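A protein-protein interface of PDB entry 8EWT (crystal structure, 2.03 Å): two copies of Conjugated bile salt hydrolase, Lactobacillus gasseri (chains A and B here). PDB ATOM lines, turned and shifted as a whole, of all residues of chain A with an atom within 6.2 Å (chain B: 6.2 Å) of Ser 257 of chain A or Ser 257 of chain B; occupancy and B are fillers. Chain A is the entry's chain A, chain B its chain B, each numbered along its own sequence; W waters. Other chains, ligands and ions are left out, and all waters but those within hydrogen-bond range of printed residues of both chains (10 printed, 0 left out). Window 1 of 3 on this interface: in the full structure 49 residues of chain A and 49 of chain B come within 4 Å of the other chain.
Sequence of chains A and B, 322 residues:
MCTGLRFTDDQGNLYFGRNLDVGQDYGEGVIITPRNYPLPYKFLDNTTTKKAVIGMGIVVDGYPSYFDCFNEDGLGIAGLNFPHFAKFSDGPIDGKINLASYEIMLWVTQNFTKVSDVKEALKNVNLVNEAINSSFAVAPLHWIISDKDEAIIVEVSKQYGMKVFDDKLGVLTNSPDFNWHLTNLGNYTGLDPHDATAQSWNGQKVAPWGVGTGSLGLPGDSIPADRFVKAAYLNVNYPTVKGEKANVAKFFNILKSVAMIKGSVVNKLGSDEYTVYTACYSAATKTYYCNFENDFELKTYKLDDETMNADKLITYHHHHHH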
ATOM      1  N   GLY A 220      25.427 -27.351  33.869  1.00  0.00           N
ATOM      2  CA  GLY A 220      25.384 -26.179  33.008  1.00  0.00           C
ATOM      3  C   GLY A 220      24.607 -24.972  33.504  1.00  0.00           C
ATOM      4  O   GLY A 220      24.487 -23.980  32.780  1.00  0.00           O
ATOM      5  N   LYS A 230      32.334 -26.052  37.225  1.00  0.00           N
ATOM      6  CA  LYS A 230      32.658 -25.893  35.815  1.00  0.00           C
ATOM      7  C   LYS A 230      33.830 -24.941  35.622  1.00  0.00           C
ATOM      8  O   LYS A 230      34.732 -25.199  34.809  1.00  0.00           O
ATOM      9  CB  LYS A 230      31.431 -25.396  35.047  1.00  0.00           C
ATOM     10  CG  LYS A 230      31.724 -25.119  33.584  1.00  0.00           C
ATOM     11  CD  LYS A 230      30.494 -25.253  32.693  1.00  0.00           C
ATOM     12  CE  LYS A 230      30.858 -24.897  31.244  1.00  0.00           C
ATOM     13  NZ  LYS A 230      29.693 -25.021  30.304  1.00  0.00           N
ATOM     14  N   LEU A 234      37.330 -25.978  33.878  1.00  0.00           N
ATOM     15  CA  LEU A 234      37.834 -25.377  32.647  1.00  0.00           C
ATOM     16  C   LEU A 234      39.222 -24.779  32.854  1.00  0.00           C
ATOM     17  O   LEU A 234      40.132 -24.996  32.043  1.00  0.00           O
ATOM     18  CB  LEU A 234      36.859 -24.321  32.142  1.00  0.00           C
ATOM     19  CG  LEU A 234      35.514 -24.863  31.660  1.00  0.00           C
ATOM     20  CD1 LEU A 234      34.670 -23.722  31.074  1.00  0.00           C
ATOM     21  CD2 LEU A 234      35.672 -25.995  30.648  1.00  0.00           C
ATOM     22  N   PHE A 252      38.371 -14.588  28.494  1.00  0.00           N
ATOM     23  CA  PHE A 252      36.978 -14.356  28.131  1.00  0.00           C
ATOM     24  C   PHE A 252      36.294 -15.658  27.691  1.00  0.00           C
ATOM     25  O   PHE A 252      35.122 -15.883  28.006  1.00  0.00           O
ATOM     26  CB  PHE A 252      36.910 -13.275  27.051  1.00  0.00           C
ATOM     27  CG  PHE A 252      36.992 -11.876  27.604  1.00  0.00           C
ATOM     28  CD1 PHE A 252      38.219 -11.312  27.918  1.00  0.00           C
ATOM     29  CD2 PHE A 252      35.837 -11.142  27.849  1.00  0.00           C
ATOM     30  CE1 PHE A 252      38.292 -10.022  28.452  1.00  0.00           C
ATOM     31  CE2 PHE A 252      35.900  -9.863  28.382  1.00  0.00           C
ATOM     32  CZ  PHE A 252      37.137  -9.300  28.685  1.00  0.00           C
ATOM     33  N   ASN A 253      37.018 -16.543  27.000  1.00  0.00           N
ATOM     34  CA  ASN A 253      36.454 -17.853  26.657  1.00  0.00           C
ATOM     35  C   ASN A 253      35.922 -18.569  27.898  1.00  0.00           C
ATOM     36  O   ASN A 253      34.797 -19.086  27.906  1.00  0.00           O
ATOM     37  CB  ASN A 253      37.512 -18.723  25.974  1.00  0.00           C
ATOM     38  CG  ASN A 253      37.872 -18.233  24.587  1.00  0.00           C
ATOM     39  OD1 ASN A 253      37.088 -17.551  23.938  1.00  0.00           O
ATOM     40  ND2 ASN A 253      39.058 -18.592  24.121  1.00  0.00           N
ATOM     41  N   ILE A 254      36.718 -18.588  28.968  1.00  0.00           N
ATOM     42  CA  ILE A 254      36.326 -19.309  30.171  1.00  0.00           C
ATOM     43  C   ILE A 254      35.160 -18.606  30.866  1.00  0.00           C
ATOM     44  O   ILE A 254      34.151 -19.237  31.201  1.00  0.00           O
ATOM     45  CB  ILE A 254      37.534 -19.473  31.110  1.00  0.00           C
ATOM     46  CG1 ILE A 254      38.589 -20.384  30.472  1.00  0.00           C
ATOM     47  CG2 ILE A 254      37.083 -20.047  32.435  1.00  0.00           C
ATOM     48  CD1 ILE A 254      39.950 -20.354  31.195  1.00  0.00           C
ATOM     49  N   LEU A 255      35.267 -17.291  31.089  1.00  0.00           N
ATOM     50  CA  LEU A 255      34.217 -16.608  31.848  1.00  0.00           C
ATOM     51  C   LEU A 255      32.902 -16.509  31.072  1.00  0.00           C
ATOM     52  O   LEU A 255      31.821 -16.506  31.683  1.00  0.00           O
ATOM     53  CB  LEU A 255      34.693 -15.217  32.283  1.00  0.00           C
ATOM     54  CG  LEU A 255      35.529 -15.188  33.576  1.00  0.00           C
ATOM     55  CD1 LEU A 255      35.600 -13.793  34.153  1.00  0.00           C
ATOM     56  CD2 LEU A 255      34.964 -16.109  34.627  1.00  0.00           C
ATOM     57  N   LYS A 256      32.957 -16.415  29.739  1.00  0.00           N
ATOM     58  CA  LYS A 256      31.718 -16.397  28.960  1.00  0.00           C
ATOM     59  C   LYS A 256      31.065 -17.771  28.939  1.00  0.00           C
ATOM     60  O   LYS A 256      29.849 -17.879  28.745  1.00  0.00           O
ATOM     61  CB  LYS A 256      31.977 -15.920  27.525  1.00  0.00           C
ATOM     62  CG  LYS A 256      32.372 -14.452  27.417  1.00  0.00           C
ATOM     63  CD  LYS A 256      31.407 -13.568  28.193  1.00  0.00           C
ATOM     64  CE  LYS A 256      31.518 -12.106  27.761  1.00  0.00           C
ATOM     65  NZ  LYS A 256      30.638 -11.218  28.583  1.00  0.00           N
ATOM     66  N   SER A 257      31.860 -18.823  29.145  1.00  0.00           N
ATOM     67  CA  SER A 257      31.309 -20.167  29.254  1.00  0.00           C
ATOM     68  C   SER A 257      30.411 -20.287  30.479  1.00  0.00           C
ATOM     69  O   SER A 257      29.361 -20.940  30.429  1.00  0.00           O
ATOM     70  CB  SER A 257      32.450 -21.185  29.310  1.00  0.00           C
ATOM     71  OG  SER A 257      31.966 -22.492  29.587  1.00  0.00           O
ATOM     72  N   VAL A 258      30.793 -19.655  31.583  1.00  0.00           N
ATOM     73  CA  VAL A 258      30.019 -19.734  32.816  1.00  0.00           C
ATOM     74  C   VAL A 258      29.249 -18.440  33.084  1.00  0.00           C
ATOM     75  O   VAL A 258      28.846 -18.178  34.222  1.00  0.00           O
ATOM     76  CB  VAL A 258      30.898 -20.108  34.016  1.00  0.00           C
ATOM     77  CG1 VAL A 258      31.534 -21.485  33.794  1.00  0.00           C
ATOM     78  CG2 VAL A 258      31.931 -19.012  34.253  1.00  0.00           C
ATOM     79  N   ALA A 259      29.051 -17.620  32.060  1.00  0.00           N
ATOM     80  CA  ALA A 259      28.234 -16.432  32.227  1.00  0.00           C
ATOM     81  C   ALA A 259      26.792 -16.823  32.527  1.00  0.00           C
ATOM     82  O   ALA A 259      26.313 -17.897  32.142  1.00  0.00           O
ATOM     83  CB  ALA A 259      28.294 -15.563  30.973  1.00  0.00           C
ATOM     84  N   ILE A 261      23.148 -16.097  31.698  1.00  0.00           N
ATOM     85  CA  ILE A 261      22.615 -15.581  30.436  1.00  0.00           C
ATOM     86  C   ILE A 261      21.272 -14.898  30.672  1.00  0.00           C
ATOM     87  O   ILE A 261      20.410 -15.417  31.396  1.00  0.00           O
ATOM     88  CB  ILE A 261      22.495 -16.714  29.399  1.00  0.00           C
ATOM     89  CG1 ILE A 261      23.866 -17.372  29.197  1.00  0.00           C
ATOM     90  CG2 ILE A 261      21.983 -16.172  28.062  1.00  0.00           C
ATOM     91  CD1 ILE A 261      25.008 -16.392  28.836  1.00  0.00           C
ATOM     92  N   GLY B 220      25.928 -28.971  31.117  1.00  0.00           N
ATOM     93  CA  GLY B 220      26.950 -28.030  30.702  1.00  0.00           C
ATOM     94  C   GLY B 220      28.101 -28.585  29.895  1.00  0.00           C
ATOM     95  O   GLY B 220      29.038 -27.847  29.578  1.00  0.00           O
ATOM     96  N   LYS B 230      20.649 -26.866  25.851  1.00  0.00           N
ATOM     97  CA  LYS B 230      21.023 -25.613  26.492  1.00  0.00           C
ATOM     98  C   LYS B 230      20.830 -24.424  25.552  1.00  0.00           C
ATOM     99  O   LYS B 230      20.249 -23.403  25.943  1.00  0.00           O
ATOM    100  CB  LYS B 230      22.464 -25.679  27.010  1.00  0.00           C
ATOM    101  CG  LYS B 230      22.889 -24.369  27.692  1.00  0.00           C
ATOM    102  CD  LYS B 230      24.113 -24.523  28.596  1.00  0.00           C
ATOM    103  CE  LYS B 230      24.474 -23.157  29.214  1.00  0.00           C
ATOM    104  NZ  LYS B 230      25.654 -23.186  30.129  1.00  0.00           N
ATOM    105  N   LEU B 234      18.323 -21.305  26.161  1.00  0.00           N
ATOM    106  CA  LEU B 234      18.813 -19.930  26.193  1.00  0.00           C
ATOM    107  C   LEU B 234      18.145 -19.082  25.113  1.00  0.00           C
ATOM    108  O   LEU B 234      17.683 -17.969  25.380  1.00  0.00           O
ATOM    109  CB  LEU B 234      20.334 -19.893  26.033  1.00  0.00           C
ATOM    110  CG  LEU B 234      21.164 -20.578  27.126  1.00  0.00           C
ATOM    111  CD1 LEU B 234      22.645 -20.338  26.908  1.00  0.00           C
ATOM    112  CD2 LEU B 234      20.740 -20.113  28.508  1.00  0.00           C
ATOM    113  N   PHE B 252      26.529 -13.407  20.597  1.00  0.00           N
ATOM    114  CA  PHE B 252      27.769 -13.977  21.120  1.00  0.00           C
ATOM    115  C   PHE B 252      27.622 -14.437  22.569  1.00  0.00           C
ATOM    116  O   PHE B 252      28.286 -15.388  22.980  1.00  0.00           O
ATOM    117  CB  PHE B 252      28.916 -12.959  20.982  1.00  0.00           C
ATOM    118  CG  PHE B 252      29.568 -12.966  19.614  1.00  0.00           C
ATOM    119  CD1 PHE B 252      29.016 -12.246  18.560  1.00  0.00           C
ATOM    120  CD2 PHE B 252      30.724 -13.707  19.379  1.00  0.00           C
ATOM    121  CE1 PHE B 252      29.605 -12.266  17.280  1.00  0.00           C
ATOM    122  CE2 PHE B 252      31.322 -13.732  18.110  1.00  0.00           C
ATOM    123  CZ  PHE B 252      30.765 -13.004  17.055  1.00  0.00           C
ATOM    124  N   ASN B 253      26.777 -13.778  23.366  1.00  0.00           N
ATOM    125  CA  ASN B 253      26.522 -14.270  24.719  1.00  0.00           C
ATOM    126  C   ASN B 253      26.023 -15.715  24.699  1.00  0.00           C
ATOM    127  O   ASN B 253      26.499 -16.562  25.467  1.00  0.00           O
ATOM    128  CB  ASN B 253      25.506 -13.373  25.414  1.00  0.00           C
ATOM    129  CG  ASN B 253      26.035 -11.983  25.651  1.00  0.00           C
ATOM    130  OD1 ASN B 253      27.240 -11.795  25.785  1.00  0.00           O
ATOM    131  ND2 ASN B 253      25.138 -10.994  25.706  1.00  0.00           N
ATOM    132  N   ILE B 254      25.072 -16.015  23.816  1.00  0.00           N
ATOM    133  CA  ILE B 254      24.487 -17.346  23.770  1.00  0.00           C
ATOM    134  C   ILE B 254      25.499 -18.365  23.259  1.00  0.00           C
ATOM    135  O   ILE B 254      25.667 -19.434  23.853  1.00  0.00           O
ATOM    136  CB  ILE B 254      23.208 -17.336  22.915  1.00  0.00           C
ATOM    137  CG1 ILE B 254      22.082 -16.612  23.669  1.00  0.00           C
ATOM    138  CG2 ILE B 254      22.786 -18.763  22.557  1.00  0.00           C
ATOM    139  CD1 ILE B 254      20.913 -16.188  22.738  1.00  0.00           C
ATOM    140  N   LEU B 255      26.189 -18.055  22.157  1.00  0.00           N
ATOM    141  CA  LEU B 255      27.065 -19.055  21.553  1.00  0.00           C
ATOM    142  C   LEU B 255      28.359 -19.226  22.339  1.00  0.00           C
ATOM    143  O   LEU B 255      28.947 -20.315  22.319  1.00  0.00           O
ATOM    144  CB  LEU B 255      27.373 -18.707  20.085  1.00  0.00           C
ATOM    145  CG  LEU B 255      26.369 -19.136  19.000  1.00  0.00           C
ATOM    146  CD1 LEU B 255      26.993 -19.137  17.612  1.00  0.00           C
ATOM    147  CD2 LEU B 255      25.775 -20.534  19.292  1.00  0.00           C
ATOM    148  N   LYS B 256      28.829 -18.184  23.033  1.00  0.00           N
ATOM    149  CA  LYS B 256      29.983 -18.387  23.906  1.00  0.00           C
ATOM    150  C   LYS B 256      29.611 -19.176  25.149  1.00  0.00           C
ATOM    151  O   LYS B 256      30.479 -19.808  25.754  1.00  0.00           O
ATOM    152  CB  LYS B 256      30.617 -17.052  24.300  1.00  0.00           C
ATOM    153  CG  LYS B 256      31.261 -16.334  23.127  1.00  0.00           C
ATOM    154  CD  LYS B 256      32.274 -17.216  22.436  1.00  0.00           C
ATOM    155  CE  LYS B 256      33.221 -16.392  21.586  1.00  0.00           C
ATOM    156  NZ  LYS B 256      34.051 -17.254  20.713  1.00  0.00           N
ATOM    157  N   SER B 257      28.335 -19.169  25.522  1.00  0.00           N
ATOM    158  CA  SER B 257      27.879 -19.984  26.637  1.00  0.00           C
ATOM    159  C   SER B 257      27.962 -21.476  26.317  1.00  0.00           C
ATOM    160  O   SER B 257      28.314 -22.280  27.186  1.00  0.00           O
ATOM    161  CB  SER B 257      26.452 -19.585  27.001  1.00  0.00           C
ATOM    162  OG  SER B 257      25.957 -20.376  28.066  1.00  0.00           O
ATOM    163  N   VAL B 258      27.620 -21.878  25.093  1.00  0.00           N
ATOM    164  CA  VAL B 258      27.633 -23.296  24.725  1.00  0.00           C
ATOM    165  C   VAL B 258      28.879 -23.653  23.910  1.00  0.00           C
ATOM    166  O   VAL B 258      28.920 -24.694  23.252  1.00  0.00           O
ATOM    167  CB  VAL B 258      26.344 -23.698  23.991  1.00  0.00           C
ATOM    168  CG1 VAL B 258      25.112 -23.381  24.871  1.00  0.00           C
ATOM    169  CG2 VAL B 258      26.237 -22.973  22.680  1.00  0.00           C
ATOM    170  N   ALA B 259      29.891 -22.796  23.939  1.00  0.00           N
ATOM    171  CA  ALA B 259      31.138 -23.037  23.242  1.00  0.00           C
ATOM    172  C   ALA B 259      31.872 -24.239  23.835  1.00  0.00           C
ATOM    173  O   ALA B 259      31.710 -24.586  25.006  1.00  0.00           O
ATOM    174  CB  ALA B 259      32.024 -21.790  23.321  1.00  0.00           C
ATOM    175  N   ILE B 261      35.210 -25.531  25.098  1.00  0.00           N
ATOM    176  CA  ILE B 261      36.350 -24.807  25.649  1.00  0.00           C
ATOM    177  C   ILE B 261      37.602 -25.657  25.500  1.00  0.00           C
ATOM    178  O   ILE B 261      37.607 -26.839  25.872  1.00  0.00           O
ATOM    179  CB  ILE B 261      36.096 -24.443  27.122  1.00  0.00           C
ATOM    180  CG1 ILE B 261      34.774 -23.665  27.248  1.00  0.00           C
ATOM    181  CG2 ILE B 261      37.270 -23.653  27.699  1.00  0.00           C
ATOM    182  CD1 ILE B 261      34.686 -22.437  26.346  1.00  0.00           C
HETATM  183  O   HOH W   1      28.031 -12.845  28.171  1.00  0.00           O
HETATM  184  O   HOH W   2      27.473 -24.429  28.782  1.00  0.00           O
HETATM  185  O   HOH W   3      36.727 -16.909  21.470  1.00  0.00           O
HETATM  186  O   HOH W   4      27.740 -23.065  31.532  1.00  0.00           O
HETATM  187  O   HOH W   5      28.199 -15.723  27.577  1.00  0.00           O
HETATM  188  O   HOH W   6      34.931 -19.419  23.154  1.00  0.00           O
HETATM  189  O   HOH W   7      26.915 -20.096  30.557  1.00  0.00           O
HETATM  190  O   HOH W   8      30.297 -23.842  27.359  1.00  0.00           O
HETATM  191  O   HOH W   9      33.264 -19.186  25.470  1.00  0.00           O
HETATM  192  O   HOH W  10      28.813  -9.867  26.843  1.00  0.00           O
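Water W3 bridges OD1 of Asn 253 of chain A (2.6 Å) and NZ of Lys 256 of chain B (2.8 Å).
Water W2 lies within hydrogen-bond range of the side-chain amino group of Lys 230 of chain B (2.6 Å), the side-chain amino group of Lys 230 of chain A (2.8 Å) and the backbone carbonyl oxygen of Ser 257 of chain B (2.8 Å).
Water W7 lies within hydrogen-bond range of O of Ser 257 of chain A, OG of Ser 257 of chain B, O of Ala 259 of chain A and NZ of Lys 230 of chain B.
Water W1 bridges OD1 of Asn 253 of chain B (2.7 Å) and NZ of Lys 256 of chain A (3.1 Å).
Water W9 lies within hydrogen-bond range of the backbone carbonyl oxygen of Lys 256 of chain B (2.9 Å) and the backbone carbonyl oxygen of Asn 253 of chain A (2.9 Å).
Water W6 bridges the side-chain amide oxygen of Asn 253 of chain A (3.0 Å) and the side-chain amino group of Lys 256 of chain B (3.4 Å).
NZ of Lys 230 of chain A lies close to OG of Ser 257 of chain A (3.5 Å).
OG of Ser 257 of chain B sits close to NZ of Lys 230 of chain B, 3.5 Å away.
Gly 220 of chain A touches its own counterpart, Gly 220 of chain B.
Gly 220 of chain A touches Lys 230 of chain B, and with the chains exchanged Lys 230 of chain A touches Gly 220 of chain B.
Lys 256 of chain B touches its own counterpart, Lys 256 of chain A.
Lys 256 of chain A touches Ser 257 of chain B, and with the chains exchanged Ser 257 of chain A touches Lys 256 of chain B.
12 positions are printed for both chains.
Of the 13 pairs that touch across the chains among the printed residues, 13 have their exchanged pair printed and touching as well.
Hydrophobic or aromatic side chains of chain A within 4 Å of the printed part of chain B: Leu 234 and Ile 261.
Printed residues of chain B that touch a printed residue of chain A: Gly 220, Lys 230, Leu 234, Asn 253, Lys 256, Ser 257 and Ile 261.
Hydrophobic or aromatic side chains of chain B that line the printed part of chain A: Leu 234 and Ile 261.
Among the printed residues, 13 pairs touch across the chains.
Ile 261 of chain B touches Leu 234 of chain A.
Ile 261 of chain B touches Asn 253 of chain A (CD1 to O, 3.7 Å).
Lys 256 of chain A touches Lys 256 of chain B.
Ser 257 of chain B touches Lys 256 of chain A.
Lys 256 of chain B touches Ser 257 of chain A.
Ser 257 of chain A touches Ser 257 of chain B.
Ser 257 of chain A touches Ile 261 of chain B (OG to CG1, 3.8 Å).
Ile 261 of chain A touches Leu 234 of chain B.
Ile 261 of chain A touches Asn 253 of chain B (CD1 to O, 3.7 Å).
CG1 of Ile 261 of chain A touches OG of Ser 257 of chain B (3.8 Å).
Of the printed residues of chain B, Ser 257 of chain A touches Lys 256 (3.6 Å), Ser 257 (3.7 Å) and Ile 261 (3.8 Å).
Of chain A, only Lys 256 (3.6 Å), Ser 257 (3.7 Å) and Ile 261 (3.8 Å) come within 4 Å of Ser 257 of chain B.
Printed residues of chain A within 4 Å of Gly 220 of chain B: Gly 220 (3.2 Å) and Lys 230 (3.0 Å).
Of the printed residues of chain B, Gly 220 of chain A touches Gly 220 (3.2 Å) and Lys 230 (3.0 Å).
Of the printed residues of chain A, Ile 261 of chain B touches Leu 234, Asn 253 and Ser 257.
The nearest residue of chain B that does not touch Ser 257 of chain A is Lys 230 of chain B (4.3 Å).
The nearest printed residue of chain B that does not touch Leu 234 of chain A is Ala 259 of chain B (6.8 Å).
The backbone carbonyl oxygen (O) of Gly 220 of chain A is in hydrogen-bond range of the side-chain amino group (NZ) of Lys 230 of chain B.
The backbone carbonyl oxygen (O) of Gly 220 of chain B sits at hydrogen-bond distance from the side-chain amino group (NZ) of Lys 230 of chain A (3.0 Å).
The backbone NH (N) of Gly 220 of chain A lies close to the backbone NH (N) of Gly 220 of chain B, at 3.2 Å.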
